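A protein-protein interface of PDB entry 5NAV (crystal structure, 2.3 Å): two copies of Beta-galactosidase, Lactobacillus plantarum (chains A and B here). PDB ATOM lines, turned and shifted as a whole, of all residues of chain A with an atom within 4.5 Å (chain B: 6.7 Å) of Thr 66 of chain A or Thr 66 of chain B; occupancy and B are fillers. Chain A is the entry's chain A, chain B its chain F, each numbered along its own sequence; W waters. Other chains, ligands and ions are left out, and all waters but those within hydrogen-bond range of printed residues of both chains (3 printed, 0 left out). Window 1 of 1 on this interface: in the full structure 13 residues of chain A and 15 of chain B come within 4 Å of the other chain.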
ATOM      1  N   THR A  35      -3.487  -5.631  15.796  1.00  0.00           N
ATOM      2  CA  THR A  35      -2.226  -5.910  15.103  1.00  0.00           C
ATOM      3  C   THR A  35      -1.461  -4.667  14.699  1.00  0.00           C
ATOM      4  O   THR A  35      -0.230  -4.633  14.845  1.00  0.00           O
ATOM      5  CB  THR A  35      -2.480  -6.732  13.840  1.00  0.00           C
ATOM      6  OG1 THR A  35      -3.431  -6.035  13.020  1.00  0.00           O
ATOM      7  CG2 THR A  35      -3.034  -8.096  14.203  1.00  0.00           C
ATOM      8  N   GLU A  36      -2.155  -3.641  14.196  1.00  0.00           N
ATOM      9  CA  GLU A  36      -1.469  -2.542  13.521  1.00  0.00           C
ATOM     10  C   GLU A  36      -0.579  -1.764  14.477  1.00  0.00           C
ATOM     11  O   GLU A  36       0.522  -1.343  14.104  1.00  0.00           O
ATOM     12  CB  GLU A  36      -2.478  -1.595  12.860  1.00  0.00           C
ATOM     13  CG  GLU A  36      -3.387  -2.263  11.818  1.00  0.00           C
ATOM     14  CD  GLU A  36      -4.468  -1.334  11.263  1.00  0.00           C
ATOM     15  OE1 GLU A  36      -4.608  -0.213  11.804  1.00  0.00           O
ATOM     16  OE2 GLU A  36      -5.212  -1.765  10.345  1.00  0.00           O
ATOM     17  N   GLY A  37      -1.023  -1.579  15.718  1.00  0.00           N
ATOM     18  CA  GLY A  37      -0.551  -0.461  16.504  1.00  0.00           C
ATOM     19  C   GLY A  37      -1.200   0.829  16.018  1.00  0.00           C
ATOM     20  O   GLY A  37      -1.859   0.892  14.968  1.00  0.00           O
ATOM     21  N   PHE A  39       0.242   3.716  15.232  1.00  0.00           N
ATOM     22  CA  PHE A  39       1.168   4.612  14.559  1.00  0.00           C
ATOM     23  C   PHE A  39       0.430   5.537  13.592  1.00  0.00           C
ATOM     24  O   PHE A  39      -0.259   5.081  12.680  1.00  0.00           O
ATOM     25  CB  PHE A  39       2.223   3.780  13.823  1.00  0.00           C
ATOM     26  CG  PHE A  39       2.968   2.813  14.717  1.00  0.00           C
ATOM     27  CD1 PHE A  39       4.085   3.228  15.448  1.00  0.00           C
ATOM     28  CD2 PHE A  39       2.571   1.488  14.810  1.00  0.00           C
ATOM     29  CE1 PHE A  39       4.773   2.340  16.270  1.00  0.00           C
ATOM     30  CE2 PHE A  39       3.266   0.584  15.632  1.00  0.00           C
ATOM     31  CZ  PHE A  39       4.364   1.007  16.356  1.00  0.00           C
ATOM     32  N   PRO A  64      -2.894  -0.863  22.996  1.00  0.00           N
ATOM     33  CA  PRO A  64      -2.844  -1.118  21.546  1.00  0.00           C
ATOM     34  C   PRO A  64      -1.893  -0.232  20.757  1.00  0.00           C
ATOM     35  O   PRO A  64      -1.870  -0.348  19.522  1.00  0.00           O
ATOM     36  CB  PRO A  64      -4.291  -0.824  21.111  1.00  0.00           C
ATOM     37  CG  PRO A  64      -4.673   0.333  22.014  1.00  0.00           C
ATOM     38  CD  PRO A  64      -4.028   0.011  23.364  1.00  0.00           C
ATOM     39  N   ASP A  65      -1.129   0.653  21.417  1.00  0.00           N
ATOM     40  CA  ASP A  65      -0.371   1.660  20.674  1.00  0.00           C
ATOM     41  C   ASP A  65       0.708   1.040  19.791  1.00  0.00           C
ATOM     42  O   ASP A  65       1.017   1.587  18.725  1.00  0.00           O
ATOM     43  CB  ASP A  65       0.236   2.690  21.622  1.00  0.00           C
ATOM     44  CG  ASP A  65      -0.809   3.346  22.538  1.00  0.00           C
ATOM     45  OD1 ASP A  65      -1.978   3.465  22.123  1.00  0.00           O
ATOM     46  OD2 ASP A  65      -0.437   3.843  23.632  1.00  0.00           O
ATOM     47  N   THR A  66       1.273  -0.103  20.184  1.00  0.00           N
ATOM     48  CA  THR A  66       2.177  -0.832  19.292  1.00  0.00           C
ATOM     49  C   THR A  66       1.615  -2.165  18.820  1.00  0.00           C
ATOM     50  O   THR A  66       1.770  -2.510  17.636  1.00  0.00           O
ATOM     51  CB  THR A  66       3.538  -1.045  19.967  1.00  0.00           C
ATOM     52  OG1 THR A  66       4.204   0.214  20.053  1.00  0.00           O
ATOM     53  CG2 THR A  66       4.424  -1.975  19.146  1.00  0.00           C
ATOM     54  N   ALA A  67       0.947  -2.911  19.698  1.00  0.00           N
ATOM     55  CA  ALA A  67       0.271  -4.162  19.334  1.00  0.00           C
ATOM     56  C   ALA A  67       1.335  -5.077  18.731  1.00  0.00           C
ATOM     57  O   ALA A  67       2.431  -5.187  19.304  1.00  0.00           O
ATOM     58  CB  ALA A  67      -0.930  -3.859  18.429  1.00  0.00           C
ATOM     59  N   SER A  68       1.087  -5.711  17.581  1.00  0.00           N
ATOM     60  CA  SER A  68       2.076  -6.559  16.929  1.00  0.00           C
ATOM     61  C   SER A  68       2.756  -5.870  15.742  1.00  0.00           C
ATOM     62  O   SER A  68       3.211  -6.538  14.807  1.00  0.00           O
ATOM     63  CB  SER A  68       1.426  -7.879  16.524  1.00  0.00           C
ATOM     64  OG  SER A  68       1.169  -8.666  17.700  1.00  0.00           O
ATOM     65  N   ASN A  69       2.833  -4.533  15.770  1.00  0.00           N
ATOM     66  CA  ASN A  69       3.655  -3.742  14.849  1.00  0.00           C
ATOM     67  C   ASN A  69       3.279  -3.941  13.373  1.00  0.00           C
ATOM     68  O   ASN A  69       4.113  -3.731  12.478  1.00  0.00           O
ATOM     69  CB  ASN A  69       5.138  -4.048  15.067  1.00  0.00           C
ATOM     70  CG  ASN A  69       6.058  -2.963  14.520  1.00  0.00           C
ATOM     71  OD1 ASN A  69       5.749  -1.765  14.581  1.00  0.00           O
ATOM     72  ND2 ASN A  69       7.207  -3.386  13.985  1.00  0.00           N
ATOM     73  N   GLN A 457       9.358  -7.205  18.670  1.00  0.00           N
ATOM     74  CA  GLN A 457       8.498  -7.497  17.511  1.00  0.00           C
ATOM     75  C   GLN A 457       9.166  -8.476  16.543  1.00  0.00           C
ATOM     76  O   GLN A 457       8.987  -8.398  15.325  1.00  0.00           O
ATOM     77  CB  GLN A 457       8.083  -6.219  16.776  1.00  0.00           C
ATOM     78  CG  GLN A 457       7.270  -5.258  17.622  1.00  0.00           C
ATOM     79  CD  GLN A 457       5.909  -5.826  17.988  1.00  0.00           C
ATOM     80  OE1 GLN A 457       5.357  -6.660  17.271  1.00  0.00           O
ATOM     81  NE2 GLN A 457       5.380  -5.399  19.128  1.00  0.00           N
ATOM     82  N   GLN B  34      17.006   5.662  24.184  1.00  0.00           N
ATOM     83  CA  GLN B  34      15.863   6.478  24.563  1.00  0.00           C
ATOM     84  C   GLN B  34      14.972   6.854  23.379  1.00  0.00           C
ATOM     85  O   GLN B  34      13.930   7.480  23.592  1.00  0.00           O
ATOM     86  CB  GLN B  34      16.347   7.739  25.300  1.00  0.00           C
ATOM     87  CG  GLN B  34      17.262   7.420  26.503  1.00  0.00           C
ATOM     88  CD  GLN B  34      17.722   8.661  27.251  1.00  0.00           C
ATOM     89  OE1 GLN B  34      18.860   9.105  27.104  1.00  0.00           O
ATOM     90  NE2 GLN B  34      16.839   9.219  28.070  1.00  0.00           N
ATOM     91  N   THR B  35      15.327   6.457  22.148  1.00  0.00           N
ATOM     92  CA  THR B  35      14.564   6.895  20.975  1.00  0.00           C
ATOM     93  C   THR B  35      14.175   5.778  20.024  1.00  0.00           C
ATOM     94  O   THR B  35      13.097   5.849  19.421  1.00  0.00           O
ATOM     95  CB  THR B  35      15.358   7.930  20.166  1.00  0.00           C
ATOM     96  OG1 THR B  35      16.614   7.357  19.797  1.00  0.00           O
ATOM     97  CG2 THR B  35      15.588   9.185  20.978  1.00  0.00           C
ATOM     98  N   GLU B  36      15.044   4.779  19.829  1.00  0.00           N
ATOM     99  CA  GLU B  36      14.898   3.878  18.684  1.00  0.00           C
ATOM    100  C   GLU B  36      13.695   2.962  18.833  1.00  0.00           C
ATOM    101  O   GLU B  36      13.010   2.666  17.845  1.00  0.00           O
ATOM    102  CB  GLU B  36      16.160   3.026  18.499  1.00  0.00           C
ATOM    103  CG  GLU B  36      17.396   3.751  17.982  1.00  0.00           C
ATOM    104  CD  GLU B  36      18.635   2.907  18.141  1.00  0.00           C
ATOM    105  OE1 GLU B  36      19.754   3.419  17.938  1.00  0.00           O
ATOM    106  OE2 GLU B  36      18.493   1.720  18.491  1.00  0.00           O
ATOM    107  N   GLY B  37      13.426   2.508  20.055  1.00  0.00           N
ATOM    108  CA  GLY B  37      12.660   1.302  20.269  1.00  0.00           C
ATOM    109  C   GLY B  37      13.555   0.088  20.082  1.00  0.00           C
ATOM    110  O   GLY B  37      14.658   0.159  19.529  1.00  0.00           O
ATOM    111  N   ASN B  38      13.075  -1.051  20.568  1.00  0.00           N
ATOM    112  CA  ASN B  38      13.813  -2.302  20.470  1.00  0.00           C
ATOM    113  C   ASN B  38      13.444  -3.126  19.234  1.00  0.00           C
ATOM    114  O   ASN B  38      13.828  -4.302  19.154  1.00  0.00           O
ATOM    115  CB  ASN B  38      13.599  -3.128  21.737  1.00  0.00           C
ATOM    116  CG  ASN B  38      14.394  -2.597  22.900  1.00  0.00           C
ATOM    117  OD1 ASN B  38      15.473  -2.030  22.710  1.00  0.00           O
ATOM    118  ND2 ASN B  38      13.870  -2.762  24.108  1.00  0.00           N
ATOM    119  N   PHE B  39      12.716  -2.545  18.282  1.00  0.00           N
ATOM    120  CA  PHE B  39      12.365  -3.240  17.044  1.00  0.00           C
ATOM    121  C   PHE B  39      13.570  -3.966  16.445  1.00  0.00           C
ATOM    122  O   PHE B  39      14.562  -3.335  16.072  1.00  0.00           O
ATOM    123  CB  PHE B  39      11.821  -2.231  16.032  1.00  0.00           C
ATOM    124  CG  PHE B  39      10.649  -1.427  16.533  1.00  0.00           C
ATOM    125  CD1 PHE B  39      10.832  -0.159  17.053  1.00  0.00           C
ATOM    126  CD2 PHE B  39       9.365  -1.936  16.472  1.00  0.00           C
ATOM    127  CE1 PHE B  39       9.755   0.591  17.514  1.00  0.00           C
ATOM    128  CE2 PHE B  39       8.271  -1.189  16.925  1.00  0.00           C
ATOM    129  CZ  PHE B  39       8.463   0.078  17.424  1.00  0.00           C
ATOM    130  N   GLY B  63       8.183   1.009  28.953  1.00  0.00           N
ATOM    131  CA  GLY B  63       9.585   0.698  28.837  1.00  0.00           C
ATOM    132  C   GLY B  63      10.196   1.267  27.575  1.00  0.00           C
ATOM    133  O   GLY B  63       9.668   2.195  26.954  1.00  0.00           O
ATOM    134  N   PRO B  64      11.334   0.702  27.175  1.00  0.00           N
ATOM    135  CA  PRO B  64      12.066   1.138  25.975  1.00  0.00           C
ATOM    136  C   PRO B  64      11.637   0.492  24.665  1.00  0.00           C
ATOM    137  O   PRO B  64      12.271   0.768  23.638  1.00  0.00           O
ATOM    138  CB  PRO B  64      13.501   0.689  26.306  1.00  0.00           C
ATOM    139  CG  PRO B  64      13.289  -0.583  27.094  1.00  0.00           C
ATOM    140  CD  PRO B  64      12.071  -0.303  27.953  1.00  0.00           C
ATOM    141  N   ASP B  65      10.641  -0.400  24.666  1.00  0.00           N
ATOM    142  CA  ASP B  65      10.428  -1.265  23.502  1.00  0.00           C
ATOM    143  C   ASP B  65       9.974  -0.489  22.269  1.00  0.00           C
ATOM    144  O   ASP B  65      10.298  -0.883  21.136  1.00  0.00           O
ATOM    145  CB  ASP B  65       9.416  -2.358  23.844  1.00  0.00           C
ATOM    146  CG  ASP B  65       9.926  -3.308  24.941  1.00  0.00           C
ATOM    147  OD1 ASP B  65      11.139  -3.347  25.228  1.00  0.00           O
ATOM    148  OD2 ASP B  65       9.086  -4.017  25.526  1.00  0.00           O
ATOM    149  N   THR B  66       9.229   0.601  22.456  1.00  0.00           N
ATOM    150  CA  THR B  66       8.898   1.502  21.350  1.00  0.00           C
ATOM    151  C   THR B  66       9.602   2.845  21.450  1.00  0.00           C
ATOM    152  O   THR B  66      10.060   3.376  20.433  1.00  0.00           O
ATOM    153  CB  THR B  66       7.382   1.722  21.277  1.00  0.00           C
ATOM    154  OG1 THR B  66       6.740   0.451  21.189  1.00  0.00           O
ATOM    155  CG2 THR B  66       6.991   2.534  20.039  1.00  0.00           C
ATOM    156  N   ALA B  67       9.732   3.379  22.664  1.00  0.00           N
ATOM    157  CA  ALA B  67      10.384   4.660  22.918  1.00  0.00           C
ATOM    158  C   ALA B  67       9.707   5.711  22.038  1.00  0.00           C
ATOM    159  O   ALA B  67       8.471   5.808  22.044  1.00  0.00           O
ATOM    160  CB  ALA B  67      11.881   4.511  22.722  1.00  0.00           C
ATOM    161  N   SER B  68      10.458   6.516  21.288  1.00  0.00           N
ATOM    162  CA  SER B  68       9.892   7.482  20.363  1.00  0.00           C
ATOM    163  C   SER B  68       9.958   6.999  18.914  1.00  0.00           C
ATOM    164  O   SER B  68       9.984   7.822  17.994  1.00  0.00           O
ATOM    165  CB  SER B  68      10.596   8.830  20.527  1.00  0.00           C
ATOM    166  OG  SER B  68      10.313   9.395  21.813  1.00  0.00           O
ATOM    167  N   ASN B  69      10.015   5.680  18.702  1.00  0.00           N
ATOM    168  CA  ASN B  69       9.805   5.071  17.389  1.00  0.00           C
ATOM    169  C   ASN B  69      10.837   5.536  16.356  1.00  0.00           C
ATOM    170  O   ASN B  69      10.566   5.545  15.159  1.00  0.00           O
ATOM    171  CB  ASN B  69       8.378   5.345  16.898  1.00  0.00           C
ATOM    172  CG  ASN B  69       7.952   4.417  15.796  1.00  0.00           C
ATOM    173  OD1 ASN B  69       8.237   3.225  15.834  1.00  0.00           O
ATOM    174  ND2 ASN B  69       7.269   4.961  14.787  1.00  0.00           N
ATOM    175  N   PHE B  70      12.036   5.934  16.794  1.00  0.00           N
ATOM    176  CA  PHE B  70      13.021   6.439  15.842  1.00  0.00           C
ATOM    177  C   PHE B  70      13.497   5.355  14.870  1.00  0.00           C
ATOM    178  O   PHE B  70      13.932   5.687  13.760  1.00  0.00           O
ATOM    179  CB  PHE B  70      14.213   7.053  16.585  1.00  0.00           C
ATOM    180  CG  PHE B  70      15.161   7.849  15.700  1.00  0.00           C
ATOM    181  CD1 PHE B  70      14.726   8.996  15.046  1.00  0.00           C
ATOM    182  CD2 PHE B  70      16.499   7.489  15.570  1.00  0.00           C
ATOM    183  CE1 PHE B  70      15.599   9.758  14.248  1.00  0.00           C
ATOM    184  CE2 PHE B  70      17.382   8.254  14.768  1.00  0.00           C
ATOM    185  CZ  PHE B  70      16.921   9.388  14.115  1.00  0.00           C
ATOM    186  N   TYR B  71      13.404   4.073  15.251  1.00  0.00           N
ATOM    187  CA  TYR B  71      13.771   3.005  14.326  1.00  0.00           C
ATOM    188  C   TYR B  71      12.929   3.055  13.059  1.00  0.00           C
ATOM    189  O   TYR B  71      13.432   2.787  11.963  1.00  0.00           O
ATOM    190  CB  TYR B  71      13.622   1.640  14.994  1.00  0.00           C
ATOM    191  CG  TYR B  71      14.015   0.485  14.106  1.00  0.00           C
ATOM    192  CD1 TYR B  71      15.346   0.104  13.976  1.00  0.00           C
ATOM    193  CD2 TYR B  71      13.057  -0.223  13.395  1.00  0.00           C
ATOM    194  CE1 TYR B  71      15.711  -0.953  13.160  1.00  0.00           C
ATOM    195  CE2 TYR B  71      13.406  -1.276  12.584  1.00  0.00           C
ATOM    196  CZ  TYR B  71      14.734  -1.639  12.469  1.00  0.00           C
ATOM    197  OH  TYR B  71      15.070  -2.692  11.648  1.00  0.00           O
ATOM    198  N   ASN B  72      11.644   3.379  13.183  1.00  0.00           N
ATOM    199  CA  ASN B  72      10.775   3.390  12.017  1.00  0.00           C
ATOM    200  C   ASN B  72      10.618   4.761  11.380  1.00  0.00           C
ATOM    201  O   ASN B  72      10.408   4.841  10.167  1.00  0.00           O
ATOM    202  CB  ASN B  72       9.386   2.847  12.380  1.00  0.00           C
ATOM    203  CG  ASN B  72       9.425   1.395  12.798  1.00  0.00           C
ATOM    204  OD1 ASN B  72       9.699   0.507  11.981  1.00  0.00           O
ATOM    205  ND2 ASN B  72       9.165   1.140  14.075  1.00  0.00           N
ATOM    206  N   TYR B 443       8.072   8.779  30.163  1.00  0.00           N
ATOM    207  CA  TYR B 443       7.620  10.039  29.583  1.00  0.00           C
ATOM    208  C   TYR B 443       6.897  10.928  30.588  1.00  0.00           C
ATOM    209  O   TYR B 443       6.104  11.791  30.187  1.00  0.00           O
ATOM    210  CB  TYR B 443       6.737   9.772  28.358  1.00  0.00           C
ATOM    211  CG  TYR B 443       7.539   9.257  27.186  1.00  0.00           C
ATOM    212  CD1 TYR B 443       7.789   7.895  27.036  1.00  0.00           C
ATOM    213  CD2 TYR B 443       8.073  10.135  26.243  1.00  0.00           C
ATOM    214  CE1 TYR B 443       8.528   7.415  25.974  1.00  0.00           C
ATOM    215  CE2 TYR B 443       8.814   9.662  25.171  1.00  0.00           C
ATOM    216  CZ  TYR B 443       9.041   8.299  25.050  1.00  0.00           C
ATOM    217  OH  TYR B 443       9.792   7.813  24.009  1.00  0.00           O
ATOM    218  N   ILE B 454       2.980   9.802  22.400  1.00  0.00           N
ATOM    219  CA  ILE B 454       3.537   8.452  22.331  1.00  0.00           C
ATOM    220  C   ILE B 454       2.486   7.378  22.081  1.00  0.00           C
ATOM    221  O   ILE B 454       2.853   6.228  21.825  1.00  0.00           O
ATOM    222  CB  ILE B 454       4.321   8.092  23.610  1.00  0.00           C
ATOM    223  CG1 ILE B 454       3.368   7.856  24.785  1.00  0.00           C
ATOM    224  CG2 ILE B 454       5.327   9.186  23.974  1.00  0.00           C
ATOM    225  CD1 ILE B 454       4.099   7.299  26.028  1.00  0.00           C
ATOM    226  N   HIS B 455       1.189   7.708  22.162  1.00  0.00           N
ATOM    227  CA  HIS B 455       0.173   6.752  21.734  1.00  0.00           C
ATOM    228  C   HIS B 455       0.230   6.535  20.224  1.00  0.00           C
ATOM    229  O   HIS B 455       0.198   5.391  19.763  1.00  0.00           O
ATOM    230  CB  HIS B 455      -1.231   7.209  22.157  1.00  0.00           C
ATOM    231  CG  HIS B 455      -1.420   7.307  23.642  1.00  0.00           C
ATOM    232  ND1 HIS B 455      -1.286   6.222  24.485  1.00  0.00           N
ATOM    233  CD2 HIS B 455      -1.733   8.359  24.437  1.00  0.00           C
ATOM    234  CE1 HIS B 455      -1.496   6.604  25.733  1.00  0.00           C
ATOM    235  NE2 HIS B 455      -1.773   7.895  25.732  1.00  0.00           N
ATOM    236  N   GLN B 457       2.753   8.063  18.205  1.00  0.00           N
ATOM    237  CA  GLN B 457       4.074   8.491  17.732  1.00  0.00           C
ATOM    238  C   GLN B 457       3.979   9.660  16.748  1.00  0.00           C
ATOM    239  O   GLN B 457       4.806   9.801  15.846  1.00  0.00           O
ATOM    240  CB  GLN B 457       4.852   7.321  17.119  1.00  0.00           C
ATOM    241  CG  GLN B 457       5.154   6.214  18.103  1.00  0.00           C
ATOM    242  CD  GLN B 457       6.076   6.675  19.219  1.00  0.00           C
ATOM    243  OE1 GLN B 457       6.901   7.574  19.043  1.00  0.00           O
ATOM    244  NE2 GLN B 457       5.919   6.075  20.380  1.00  0.00           N
HETATM  245  O   HOH W   1       2.175   4.102  18.157  1.00  0.00           O
HETATM  246  O   HOH W   2       9.641  -2.227  12.713  1.00  0.00           O
HETATM  247  O   HOH W   3      -3.935   5.044  23.215  1.00  0.00           O
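Of chain B, only Thr 66 comes within 4 Å of Thr 66 of chain A.
Thr 66 of chain B touches one residue of chain A.
Of the printed residues of chain A, Asn 69 of chain B touches Phe 39 (3.6 Å).
Printed residues of chain A within 4 Å of Phe 39 of chain B: Asn 69.
Ala 67 of chain B touches none of the printed residues of chain A.
The nearest residue of chain A that does not touch Thr 66 of chain B is Phe 39 of chain A (4.4 Å).
The nearest printed residue of chain B that does not touch Phe 39 of chain A is Gln 457 of chain B (4.1 Å).
Water W3 lies within hydrogen-bond range of OD1 of Asp 65 of chain A (2.7 Å) and ND1 of His 455 of chain B (3.2 Å).
Water W1 bridges O of Asp 65 of chain A (2.8 Å) and O of His 455 of chain B (2.9 Å).
Water W2 bridges the side-chain amide oxygen of Asn 72 of chain B (2.8 Å) and the side-chain amide nitrogen of Asn 69 of chain A (3.0 Å).
Phe 39 of chain A touches Asn 69 of chain B, and with the chains exchanged Asn 69 of chain A touches Phe 39 of chain B.
Thr 66 of chain B touches its own counterpart, Thr 66 of chain A.
11 positions are printed for both chains.
OD2 of Asp 65 of chain A is in hydrogen-bond range of ND1 of His 455 of chain B, 2.7 Å away.
The side-chain hydroxyl (OG1) of Thr 66 of chain A sits at hydrogen-bond distance from the side-chain hydroxyl (OG1) of Thr 66 of chain B.
Phe 39 of chain A touches Asn 69 of chain B (CE1 to OD1, 3.6 Å).
Asn 69 of chain A touches Phe 39 of chain B (OD1 to CE2, 3.5 Å).
O of Thr 35 of chain B is in hydrogen-bond range of N of Asn 69 of chain B (3.2 Å).
The side-chain amide oxygen (OD1) of Asn 69 of chain B is in hydrogen-bond range of the side-chain amide nitrogen (ND2) of Asn 72 of chain B (2.9 Å).
The backbone carbonyl oxygen of Thr 35 of chain A lies within hydrogen-bond range of the backbone NH of Asn 69 of chain A, 3.2 Å away.
N of Gly 37 of chain B sits close to O of Thr 66 of chain B (3.5 Å).
Printed residues of chain B that touch a printed residue of chain A: Phe 39, Thr 66, Asn 69 and His 455.
Along chain B the printed residues that touch a printed residue of chain A span positions 39 to 455.
Printed residues of chain A that touch a printed residue of chain B: Phe 39, Asp 65, Thr 66 and Asn 69.
Among the printed residues, 4 pairs touch across the chains.
Among the printed residues, no Asp or Glu carboxylate lies within 4 Å of a Lys or Arg side-chain nitrogen of the other chain.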
